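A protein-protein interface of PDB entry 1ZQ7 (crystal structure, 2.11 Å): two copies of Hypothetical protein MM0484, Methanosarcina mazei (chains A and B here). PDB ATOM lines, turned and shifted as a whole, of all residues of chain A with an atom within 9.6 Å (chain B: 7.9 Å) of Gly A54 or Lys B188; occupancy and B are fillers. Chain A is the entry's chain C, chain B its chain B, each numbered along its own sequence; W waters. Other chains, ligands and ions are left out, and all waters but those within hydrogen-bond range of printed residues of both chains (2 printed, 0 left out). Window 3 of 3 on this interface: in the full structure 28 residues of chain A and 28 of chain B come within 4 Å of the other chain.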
ATOM      1  N   LEU A  51     -25.993  -8.938 -19.596  1.00  0.00           N
ATOM      2  CA  LEU A  51     -25.941  -9.072 -18.152  1.00  0.00           C
ATOM      3  C   LEU A  51     -24.646  -8.440 -17.688  1.00  0.00           C
ATOM      4  O   LEU A  51     -23.619  -8.596 -18.345  1.00  0.00           O
ATOM      5  CB  LEU A  51     -25.926 -10.546 -17.746  1.00  0.00           C
ATOM      6  CG  LEU A  51     -27.074 -11.448 -18.214  1.00  0.00           C
ATOM      7  CD1 LEU A  51     -26.774 -12.878 -17.800  1.00  0.00           C
ATOM      8  CD2 LEU A  51     -28.401 -10.965 -17.622  1.00  0.00           C
ATOM      9  N   THR A  52     -24.699  -7.706 -16.581  1.00  0.00           N
ATOM     10  CA  THR A  52     -23.492  -7.108 -16.001  1.00  0.00           C
ATOM     11  C   THR A  52     -23.491  -7.460 -14.520  1.00  0.00           C
ATOM     12  O   THR A  52     -24.541  -7.730 -13.941  1.00  0.00           O
ATOM     13  CB  THR A  52     -23.450  -5.558 -16.109  1.00  0.00           C
ATOM     14  OG1 THR A  52     -24.538  -4.992 -15.370  1.00  0.00           O
ATOM     15  CG2 THR A  52     -23.526  -5.114 -17.559  1.00  0.00           C
ATOM     16  N   GLU A  53     -22.309  -7.471 -13.918  1.00  0.00           N
ATOM     17  CA  GLU A  53     -22.163  -7.763 -12.501  1.00  0.00           C
ATOM     18  C   GLU A  53     -21.020  -6.904 -11.968  1.00  0.00           C
ATOM     19  O   GLU A  53     -19.869  -7.041 -12.399  1.00  0.00           O
ATOM     20  CB  GLU A  53     -21.855  -9.245 -12.288  1.00  0.00           C
ATOM     21  CG  GLU A  53     -21.751  -9.664 -10.828  1.00  0.00           C
ATOM     22  CD  GLU A  53     -21.792 -11.173 -10.661  1.00  0.00           C
ATOM     23  OE1 GLU A  53     -20.994 -11.869 -11.318  1.00  0.00           O
ATOM     24  OE2 GLU A  53     -22.624 -11.666  -9.874  1.00  0.00           O
ATOM     25  N   GLY A  54     -21.344  -6.003 -11.044  1.00  0.00           N
ATOM     26  CA  GLY A  54     -20.328  -5.132 -10.480  1.00  0.00           C
ATOM     27  C   GLY A  54     -19.746  -4.174 -11.503  1.00  0.00           C
ATOM     28  O   GLY A  54     -18.561  -3.850 -11.447  1.00  0.00           O
ATOM     29  N   GLY A  55     -20.584  -3.723 -12.437  1.00  0.00           N
ATOM     30  CA  GLY A  55     -20.147  -2.805 -13.475  1.00  0.00           C
ATOM     31  C   GLY A  55     -19.406  -3.468 -14.629  1.00  0.00           C
ATOM     32  O   GLY A  55     -19.050  -2.811 -15.611  1.00  0.00           O
ATOM     33  N   LEU A  56     -19.192  -4.777 -14.521  1.00  0.00           N
ATOM     34  CA  LEU A  56     -18.475  -5.541 -15.539  1.00  0.00           C
ATOM     35  C   LEU A  56     -19.398  -6.453 -16.340  1.00  0.00           C
ATOM     36  O   LEU A  56     -20.401  -6.932 -15.818  1.00  0.00           O
ATOM     37  CB  LEU A  56     -17.389  -6.382 -14.867  1.00  0.00           C
ATOM     38  CG  LEU A  56     -16.341  -5.592 -14.086  1.00  0.00           C
ATOM     39  CD1 LEU A  56     -15.438  -6.545 -13.294  1.00  0.00           C
ATOM     40  CD2 LEU A  56     -15.526  -4.754 -15.060  1.00  0.00           C
ATOM     41  N   LEU A  57     -19.048  -6.699 -17.604  1.00  0.00           N
ATOM     42  CA  LEU A  57     -19.851  -7.564 -18.468  1.00  0.00           C
ATOM     43  C   LEU A  57     -19.854  -8.974 -17.901  1.00  0.00           C
ATOM     44  O   LEU A  57     -18.799  -9.510 -17.572  1.00  0.00           O
ATOM     45  CB  LEU A  57     -19.282  -7.601 -19.892  1.00  0.00           C
ATOM     46  CG  LEU A  57     -20.080  -8.469 -20.881  1.00  0.00           C
ATOM     47  CD1 LEU A  57     -21.445  -7.835 -21.102  1.00  0.00           C
ATOM     48  CD2 LEU A  57     -19.342  -8.597 -22.214  1.00  0.00           C
ATOM     49  N   ARG A  58     -21.038  -9.569 -17.781  1.00  0.00           N
ATOM     50  CA  ARG A  58     -21.151 -10.923 -17.250  1.00  0.00           C
ATOM     51  C   ARG A  58     -21.643 -11.883 -18.320  1.00  0.00           C
ATOM     52  O   ARG A  58     -21.509 -13.099 -18.187  1.00  0.00           O
ATOM     53  CB  ARG A  58     -22.115 -10.963 -16.058  1.00  0.00           C
ATOM     54  CG  ARG A  58     -22.231 -12.340 -15.389  1.00  0.00           C
ATOM     55  CD  ARG A  58     -20.927 -12.703 -14.686  1.00  0.00           C
ATOM     56  NE  ARG A  58     -20.912 -14.052 -14.122  1.00  0.00           N
ATOM     57  CZ  ARG A  58     -20.938 -15.176 -14.839  1.00  0.00           C
ATOM     58  NH1 ARG A  58     -20.992 -15.125 -16.164  1.00  0.00           N
ATOM     59  NH2 ARG A  58     -20.870 -16.354 -14.230  1.00  0.00           N
ATOM     60  N   GLU A  95     -26.316 -15.764  -8.317  1.00  0.00           N
ATOM     61  CA  GLU A  95     -25.648 -14.608  -8.905  1.00  0.00           C
ATOM     62  C   GLU A  95     -26.616 -13.558  -9.443  1.00  0.00           C
ATOM     63  O   GLU A  95     -26.290 -12.372  -9.477  1.00  0.00           O
ATOM     64  CB  GLU A  95     -24.713 -15.046 -10.040  1.00  0.00           C
ATOM     65  CG  GLU A  95     -23.465 -15.778  -9.594  1.00  0.00           C
ATOM     66  CD  GLU A  95     -22.492 -15.977 -10.733  1.00  0.00           C
ATOM     67  OE1 GLU A  95     -22.039 -14.959 -11.303  1.00  0.00           O
ATOM     68  OE2 GLU A  95     -22.184 -17.143 -11.062  1.00  0.00           O
ATOM     69  N   LYS A  97     -29.013 -12.132  -8.162  1.00  0.00           N
ATOM     70  CA  LYS A  97     -29.381 -11.075  -7.230  1.00  0.00           C
ATOM     71  C   LYS A  97     -28.308  -9.992  -7.235  1.00  0.00           C
ATOM     72  O   LYS A  97     -28.502  -8.910  -6.688  1.00  0.00           O
ATOM     73  CB  LYS A  97     -29.576 -11.634  -5.814  1.00  0.00           C
ATOM     74  CG  LYS A  97     -28.392 -12.398  -5.255  1.00  0.00           C
ATOM     75  CD  LYS A  97     -28.717 -12.978  -3.881  1.00  0.00           C
ATOM     76  CE  LYS A  97     -27.548 -13.784  -3.326  1.00  0.00           C
ATOM     77  NZ  LYS A  97     -26.337 -12.938  -3.155  1.00  0.00           N
ATOM     78  N   ASN A  98     -27.184 -10.285  -7.884  1.00  0.00           N
ATOM     79  CA  ASN A  98     -26.073  -9.342  -7.969  1.00  0.00           C
ATOM     80  C   ASN A  98     -25.828  -8.914  -9.412  1.00  0.00           C
ATOM     81  O   ASN A  98     -24.821  -8.278  -9.712  1.00  0.00           O
ATOM     82  CB  ASN A  98     -24.797  -9.993  -7.440  1.00  0.00           C
ATOM     83  CG  ASN A  98     -24.918 -10.435  -6.000  1.00  0.00           C
ATOM     84  OD1 ASN A  98     -24.241 -11.375  -5.573  1.00  0.00           O
ATOM     85  ND2 ASN A  98     -25.770  -9.755  -5.236  1.00  0.00           N
ATOM     86  N   ILE A  99     -26.755  -9.257 -10.299  1.00  0.00           N
ATOM     87  CA  ILE A  99     -26.603  -8.942 -11.716  1.00  0.00           C
ATOM     88  C   ILE A  99     -27.607  -7.925 -12.248  1.00  0.00           C
ATOM     89  O   ILE A  99     -28.751  -7.885 -11.809  1.00  0.00           O
ATOM     90  CB  ILE A  99     -26.705 -10.254 -12.558  1.00  0.00           C
ATOM     91  CG1 ILE A  99     -25.457 -11.109 -12.327  1.00  0.00           C
ATOM     92  CG2 ILE A  99     -26.904  -9.934 -14.035  1.00  0.00           C
ATOM     93  CD1 ILE A  99     -25.548 -12.512 -12.904  1.00  0.00           C
ATOM     94  N   LEU A 100     -27.159  -7.084 -13.177  1.00  0.00           N
ATOM     95  CA  LEU A 100     -28.034  -6.099 -13.805  1.00  0.00           C
ATOM     96  C   LEU A 100     -28.369  -6.633 -15.194  1.00  0.00           C
ATOM     97  O   LEU A 100     -27.481  -7.101 -15.913  1.00  0.00           O
ATOM     98  CB  LEU A 100     -27.345  -4.740 -13.946  1.00  0.00           C
ATOM     99  CG  LEU A 100     -27.133  -3.836 -12.724  1.00  0.00           C
ATOM    100  CD1 LEU A 100     -28.477  -3.574 -12.054  1.00  0.00           C
ATOM    101  CD2 LEU A 100     -26.157  -4.482 -11.752  1.00  0.00           C
ATOM    102  N   VAL A 101     -29.648  -6.568 -15.556  1.00  0.00           N
ATOM    103  CA  VAL A 101     -30.120  -7.042 -16.849  1.00  0.00           C
ATOM    104  C   VAL A 101     -30.391  -5.887 -17.806  1.00  0.00           C
ATOM    105  O   VAL A 101     -31.041  -4.909 -17.446  1.00  0.00           O
ATOM    106  CB  VAL A 101     -31.420  -7.869 -16.701  1.00  0.00           C
ATOM    107  CG1 VAL A 101     -32.030  -8.147 -18.079  1.00  0.00           C
ATOM    108  CG2 VAL A 101     -31.122  -9.181 -15.992  1.00  0.00           C
ATOM    109  N   GLU A 189     -31.010  -1.292 -10.931  1.00  0.00           N
ATOM    110  CA  GLU A 189     -30.687  -2.247  -9.879  1.00  0.00           C
ATOM    111  C   GLU A 189     -31.475  -3.520 -10.126  1.00  0.00           C
ATOM    112  O   GLU A 189     -32.538  -3.489 -10.745  1.00  0.00           O
ATOM    113  CB  GLU A 189     -31.027  -1.684  -8.494  1.00  0.00           C
ATOM    114  CG  GLU A 189     -29.897  -0.875  -7.864  1.00  0.00           C
ATOM    115  CD  GLU A 189     -28.615  -1.690  -7.669  1.00  0.00           C
ATOM    116  OE1 GLU A 189     -28.015  -2.123  -8.678  1.00  0.00           O
ATOM    117  OE2 GLU A 189     -28.209  -1.898  -6.506  1.00  0.00           O
ATOM    118  N   PRO A 190     -30.965  -4.659  -9.640  1.00  0.00           N
ATOM    119  CA  PRO A 190     -31.659  -5.931  -9.838  1.00  0.00           C
ATOM    120  C   PRO A 190     -33.134  -5.895  -9.462  1.00  0.00           C
ATOM    121  O   PRO A 190     -33.499  -5.641  -8.316  1.00  0.00           O
ATOM    122  CB  PRO A 190     -30.842  -6.913  -8.996  1.00  0.00           C
ATOM    123  CG  PRO A 190     -30.153  -6.040  -7.984  1.00  0.00           C
ATOM    124  CD  PRO A 190     -29.783  -4.828  -8.781  1.00  0.00           C
ATOM    125  N   VAL B  11      -7.823   6.967 -15.540  1.00  0.00           N
ATOM    126  CA  VAL B  11      -9.128   7.536 -15.225  1.00  0.00           C
ATOM    127  C   VAL B  11      -9.003   8.761 -14.326  1.00  0.00           C
ATOM    128  O   VAL B  11      -9.698   9.753 -14.520  1.00  0.00           O
ATOM    129  CB  VAL B  11     -10.068   6.506 -14.547  1.00  0.00           C
ATOM    130  CG1 VAL B  11     -10.221   5.276 -15.435  1.00  0.00           C
ATOM    131  CG2 VAL B  11      -9.532   6.125 -13.185  1.00  0.00           C
ATOM    132  N   LEU B 100     -19.567   9.250 -13.791  1.00  0.00           N
ATOM    133  CA  LEU B 100     -18.605   8.156 -13.738  1.00  0.00           C
ATOM    134  C   LEU B 100     -17.708   8.261 -14.971  1.00  0.00           C
ATOM    135  O   LEU B 100     -18.196   8.445 -16.089  1.00  0.00           O
ATOM    136  CB  LEU B 100     -19.329   6.806 -13.745  1.00  0.00           C
ATOM    137  CG  LEU B 100     -19.382   5.990 -12.448  1.00  0.00           C
ATOM    138  CD1 LEU B 100     -19.738   6.865 -11.264  1.00  0.00           C
ATOM    139  CD2 LEU B 100     -20.409   4.869 -12.618  1.00  0.00           C
ATOM    140  N   VAL B 101     -16.403   8.136 -14.763  1.00  0.00           N
ATOM    141  CA  VAL B 101     -15.442   8.236 -15.852  1.00  0.00           C
ATOM    142  C   VAL B 101     -14.966   6.867 -16.329  1.00  0.00           C
ATOM    143  O   VAL B 101     -14.769   5.953 -15.533  1.00  0.00           O
ATOM    144  CB  VAL B 101     -14.223   9.084 -15.415  1.00  0.00           C
ATOM    145  CG1 VAL B 101     -13.177   9.129 -16.523  1.00  0.00           C
ATOM    146  CG2 VAL B 101     -14.683  10.501 -15.055  1.00  0.00           C
ATOM    147  N   PHE B 185     -10.839   0.916 -18.295  1.00  0.00           N
ATOM    148  CA  PHE B 185     -10.771   1.101 -16.855  1.00  0.00           C
ATOM    149  C   PHE B 185     -11.906   2.066 -16.571  1.00  0.00           C
ATOM    150  O   PHE B 185     -12.083   3.046 -17.291  1.00  0.00           O
ATOM    151  CB  PHE B 185      -9.426   1.699 -16.450  1.00  0.00           C
ATOM    152  CG  PHE B 185      -8.286   0.731 -16.559  1.00  0.00           C
ATOM    153  CD1 PHE B 185      -7.985  -0.130 -15.509  1.00  0.00           C
ATOM    154  CD2 PHE B 185      -7.525   0.663 -17.722  1.00  0.00           C
ATOM    155  CE1 PHE B 185      -6.937  -1.053 -15.613  1.00  0.00           C
ATOM    156  CE2 PHE B 185      -6.474  -0.256 -17.843  1.00  0.00           C
ATOM    157  CZ  PHE B 185      -6.178  -1.116 -16.788  1.00  0.00           C
ATOM    158  N   LYS B 186     -12.689   1.789 -15.540  1.00  0.00           N
ATOM    159  CA  LYS B 186     -13.809   2.655 -15.243  1.00  0.00           C
ATOM    160  C   LYS B 186     -14.068   2.808 -13.751  1.00  0.00           C
ATOM    161  O   LYS B 186     -13.767   1.918 -12.959  1.00  0.00           O
ATOM    162  CB  LYS B 186     -15.064   2.127 -15.946  1.00  0.00           C
ATOM    163  CG  LYS B 186     -15.488   0.728 -15.524  1.00  0.00           C
ATOM    164  CD  LYS B 186     -16.747   0.250 -16.264  1.00  0.00           C
ATOM    165  CE  LYS B 186     -16.505   0.070 -17.760  1.00  0.00           C
ATOM    166  NZ  LYS B 186     -17.675  -0.561 -18.453  1.00  0.00           N
ATOM    167  N   GLU B 187     -14.622   3.951 -13.377  1.00  0.00           N
ATOM    168  CA  GLU B 187     -14.928   4.215 -11.982  1.00  0.00           C
ATOM    169  C   GLU B 187     -16.133   3.396 -11.557  1.00  0.00           C
ATOM    170  O   GLU B 187     -17.109   3.287 -12.296  1.00  0.00           O
ATOM    171  CB  GLU B 187     -15.243   5.695 -11.773  1.00  0.00           C
ATOM    172  CG  GLU B 187     -14.089   6.634 -12.054  1.00  0.00           C
ATOM    173  CD  GLU B 187     -14.443   8.072 -11.742  1.00  0.00           C
ATOM    174  OE1 GLU B 187     -13.760   8.683 -10.893  1.00  0.00           O
ATOM    175  OE2 GLU B 187     -15.408   8.588 -12.347  1.00  0.00           O
ATOM    176  N   LYS B 188     -16.058   2.819 -10.365  1.00  0.00           N
ATOM    177  CA  LYS B 188     -17.163   2.039  -9.828  1.00  0.00           C
ATOM    178  C   LYS B 188     -18.098   3.046  -9.148  1.00  0.00           C
ATOM    179  O   LYS B 188     -19.309   2.849  -9.089  1.00  0.00           O
ATOM    180  CB  LYS B 188     -16.624   1.003  -8.839  1.00  0.00           C
ATOM    181  CG  LYS B 188     -17.597  -0.113  -8.500  1.00  0.00           C
ATOM    182  CD  LYS B 188     -16.860  -1.303  -7.897  1.00  0.00           C
ATOM    183  CE  LYS B 188     -17.822  -2.293  -7.265  1.00  0.00           C
ATOM    184  NZ  LYS B 188     -18.871  -2.731  -8.220  1.00  0.00           N
ATOM    185  N   GLU B 189     -17.511   4.127  -8.646  1.00  0.00           N
ATOM    186  CA  GLU B 189     -18.241   5.223  -8.008  1.00  0.00           C
ATOM    187  C   GLU B 189     -17.459   6.508  -8.303  1.00  0.00           C
ATOM    188  O   GLU B 189     -16.254   6.467  -8.542  1.00  0.00           O
ATOM    189  CB  GLU B 189     -18.343   5.030  -6.490  1.00  0.00           C
ATOM    190  CG  GLU B 189     -19.161   3.833  -6.032  1.00  0.00           C
ATOM    191  CD  GLU B 189     -19.438   3.855  -4.530  1.00  0.00           C
ATOM    192  OE1 GLU B 189     -20.283   4.662  -4.078  1.00  0.00           O
ATOM    193  OE2 GLU B 189     -18.803   3.068  -3.797  1.00  0.00           O
ATOM    194  N   PRO B 190     -18.129   7.667  -8.289  1.00  0.00           N
ATOM    195  CA  PRO B 190     -17.407   8.910  -8.570  1.00  0.00           C
ATOM    196  C   PRO B 190     -16.128   9.071  -7.751  1.00  0.00           C
ATOM    197  O   PRO B 190     -16.162   9.091  -6.517  1.00  0.00           O
ATOM    198  CB  PRO B 190     -18.444   9.984  -8.256  1.00  0.00           C
ATOM    199  CG  PRO B 190     -19.731   9.313  -8.638  1.00  0.00           C
ATOM    200  CD  PRO B 190     -19.558   7.930  -8.044  1.00  0.00           C
ATOM    201  N   ASP B 191     -15.001   9.171  -8.452  1.00  0.00           N
ATOM    202  CA  ASP B 191     -13.701   9.340  -7.823  1.00  0.00           C
ATOM    203  C   ASP B 191     -13.384   8.173  -6.893  1.00  0.00           C
ATOM    204  O   ASP B 191     -12.533   8.278  -6.005  1.00  0.00           O
ATOM    205  CB  ASP B 191     -13.664  10.663  -7.051  1.00  0.00           C
ATOM    206  CG  ASP B 191     -12.323  11.361  -7.162  1.00  0.00           C
ATOM    207  OD1 ASP B 191     -12.209  12.497  -6.677  1.00  0.00           O
ATOM    208  OD2 ASP B 191     -11.382  10.774  -7.739  1.00  0.00           O
ATOM    209  N   GLY B 192     -14.058   7.051  -7.123  1.00  0.00           N
ATOM    210  CA  GLY B 192     -13.839   5.883  -6.293  1.00  0.00           C
ATOM    211  C   GLY B 192     -12.942   4.815  -6.887  1.00  0.00           C
ATOM    212  O   GLY B 192     -11.995   5.099  -7.626  1.00  0.00           O
ATOM    213  N   GLU B 193     -13.251   3.571  -6.547  1.00  0.00           N
ATOM    214  CA  GLU B 193     -12.495   2.417  -7.005  1.00  0.00           C
ATOM    215  C   GLU B 193     -12.543   2.293  -8.522  1.00  0.00           C
ATOM    216  O   GLU B 193     -13.546   2.636  -9.151  1.00  0.00           O
ATOM    217  CB  GLU B 193     -13.076   1.152  -6.380  1.00  0.00           C
ATOM    218  CG  GLU B 193     -12.242  -0.094  -6.589  1.00  0.00           C
ATOM    219  CD  GLU B 193     -13.057  -1.361  -6.436  1.00  0.00           C
ATOM    220  OE1 GLU B 193     -14.045  -1.347  -5.668  1.00  0.00           O
ATOM    221  OE2 GLU B 193     -12.706  -2.373  -7.077  1.00  0.00           O
ATOM    222  N   VAL B 194     -11.456   1.808  -9.109  1.00  0.00           N
ATOM    223  CA  VAL B 194     -11.399   1.630 -10.556  1.00  0.00           C
ATOM    224  C   VAL B 194     -11.382   0.143 -10.877  1.00  0.00           C
ATOM    225  O   VAL B 194     -10.610  -0.620 -10.290  1.00  0.00           O
ATOM    226  CB  VAL B 194     -10.144   2.289 -11.158  1.00  0.00           C
ATOM    227  CG1 VAL B 194     -10.136   2.109 -12.677  1.00  0.00           C
ATOM    228  CG2 VAL B 194     -10.123   3.766 -10.801  1.00  0.00           C
ATOM    229  N   ILE B 195     -12.251  -0.258 -11.800  1.00  0.00           N
ATOM    230  CA  ILE B 195     -12.360  -1.649 -12.216  1.00  0.00           C
ATOM    231  C   ILE B 195     -11.948  -1.771 -13.686  1.00  0.00           C
ATOM    232  O   ILE B 195     -12.035  -0.803 -14.443  1.00  0.00           O
ATOM    233  CB  ILE B 195     -13.809  -2.167 -12.019  1.00  0.00           C
ATOM    234  CG1 ILE B 195     -14.774  -1.453 -12.967  1.00  0.00           C
ATOM    235  CG2 ILE B 195     -14.261  -1.886 -10.591  1.00  0.00           C
ATOM    236  CD1 ILE B 195     -16.215  -1.903 -12.806  1.00  0.00           C
ATOM    237  N   GLU B 196     -11.498  -2.954 -14.086  1.00  0.00           N
ATOM    238  CA  GLU B 196     -11.055  -3.179 -15.462  1.00  0.00           C
ATOM    239  C   GLU B 196     -11.970  -4.128 -16.234  1.00  0.00           C
ATOM    240  O   GLU B 196     -12.250  -5.234 -15.785  1.00  0.00           O
ATOM    241  CB  GLU B 196      -9.626  -3.747 -15.472  1.00  0.00           C
ATOM    242  CG  GLU B 196      -8.970  -3.765 -16.851  1.00  0.00           C
ATOM    243  CD  GLU B 196      -7.676  -4.579 -16.892  1.00  0.00           C
ATOM    244  OE1 GLU B 196      -6.977  -4.661 -15.859  1.00  0.00           O
ATOM    245  OE2 GLU B 196      -7.352  -5.127 -17.965  1.00  0.00           O
ATOM    246  N   GLU B 197     -12.420  -3.677 -17.401  1.00  0.00           N
ATOM    247  CA  GLU B 197     -13.285  -4.461 -18.277  1.00  0.00           C
ATOM    248  C   GLU B 197     -12.401  -4.987 -19.407  1.00  0.00           C
ATOM    249  O   GLU B 197     -11.949  -4.209 -20.251  1.00  0.00           O
ATOM    250  CB  GLU B 197     -14.387  -3.570 -18.853  1.00  0.00           C
ATOM    251  CG  GLU B 197     -15.313  -4.259 -19.847  1.00  0.00           C
ATOM    252  CD  GLU B 197     -15.974  -5.500 -19.271  1.00  0.00           C
ATOM    253  OE1 GLU B 197     -15.467  -6.610 -19.531  1.00  0.00           O
ATOM    254  OE2 GLU B 197     -16.992  -5.362 -18.551  1.00  0.00           O
HETATM  255  O   HOH W   1     -20.871  -1.209 -10.306  1.00  0.00           O
HETATM  256  O   HOH W   2     -16.228  -8.536 -18.059  1.00  0.00           O
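O of Gly A54 is in hydrogen-bond range of NZ of Lys B188, 3.4 Å away.
The backbone NH of Leu A57 lies within hydrogen-bond range of the side-chain carboxylate of Glu B197, at 2.6 Å.
N of Lys B186 lies within hydrogen-bond range of O of Ile B195, 2.9 Å away.
The backbone NH (N) of Lys B188 sits at hydrogen-bond distance from the backbone carbonyl oxygen (O) of Glu B193, at 2.8 Å.
Among the printed residues, pairs that only touch across the chains: Gly A54 with Ile B195, Gly A55 with Lys B186, Gly A55 with Ile B195, Leu A56 with Ile B195, Leu A56 with Glu B196 and Leu A56 with Glu B197.
Of the printed residues of chain B, Gly A54 touches Lys B188 (3.4 Å) and Ile B195 (3.3 Å).
Of chain A, only Gly A54 comes within 4 Å of Lys B188.
No residue of chain A comes within 4 Å of Glu B193.
Of the printed residues of chain B, Gly A55 touches Lys B186 (3.9 Å) and Ile B195 (3.99 Å).
Printed residues of chain B within 4 Å of Leu A56: Ile B195, Glu B196 and Glu B197.
Of the printed residues of chain A, Glu B197 touches Leu A56 (3.4 Å) and Leu A57 (2.6 Å).
Gly B192 touches none of the printed residues of chain A.
Glu A189 touches none of the printed residues of chain B.
The nearest residue of chain B that does not touch Gly A54 is Lys B186 (6.6 Å).
The nearest residue of chain A that does not touch Lys B188 is Gly A55 (4.7 Å).
The nearest printed residue of chain B that does not touch Leu A57 is Lys B186 (6.3 Å).
Of the 16 printed residues of chain B, 5 touch a printed residue of chain A.
Printed residues of chain B that touch a printed residue of chain A: Lys B186, Lys B188, Ile B195, Glu B196 and Glu B197.
Hydrophobic or aromatic side chains of chain B within 4 Å of the printed part of chain A: Ile B195.
Hydrophobic or aromatic side chains of chain A within 4 Å of the printed part of chain B: Leu A56 and Leu A57.
Among the printed residues, 8 pairs touch across the chains.
Among the printed residues, no Asp or Glu carboxylate lies within 4 Å of a Lys or Arg side-chain nitrogen of the other chain.
Positions printed for both chains: 100, 101, 189 and 190.
Water W2 lies within hydrogen-bond range of the side-chain carboxylate (OE1) of Glu B197 (2.5 Å) and the backbone carbonyl oxygen (O) of Leu A57 (2.8 Å).
Water W1 lies within hydrogen-bond range of NZ of Lys B188 (3.3 Å) and N of Gly A55 (3.3 Å).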
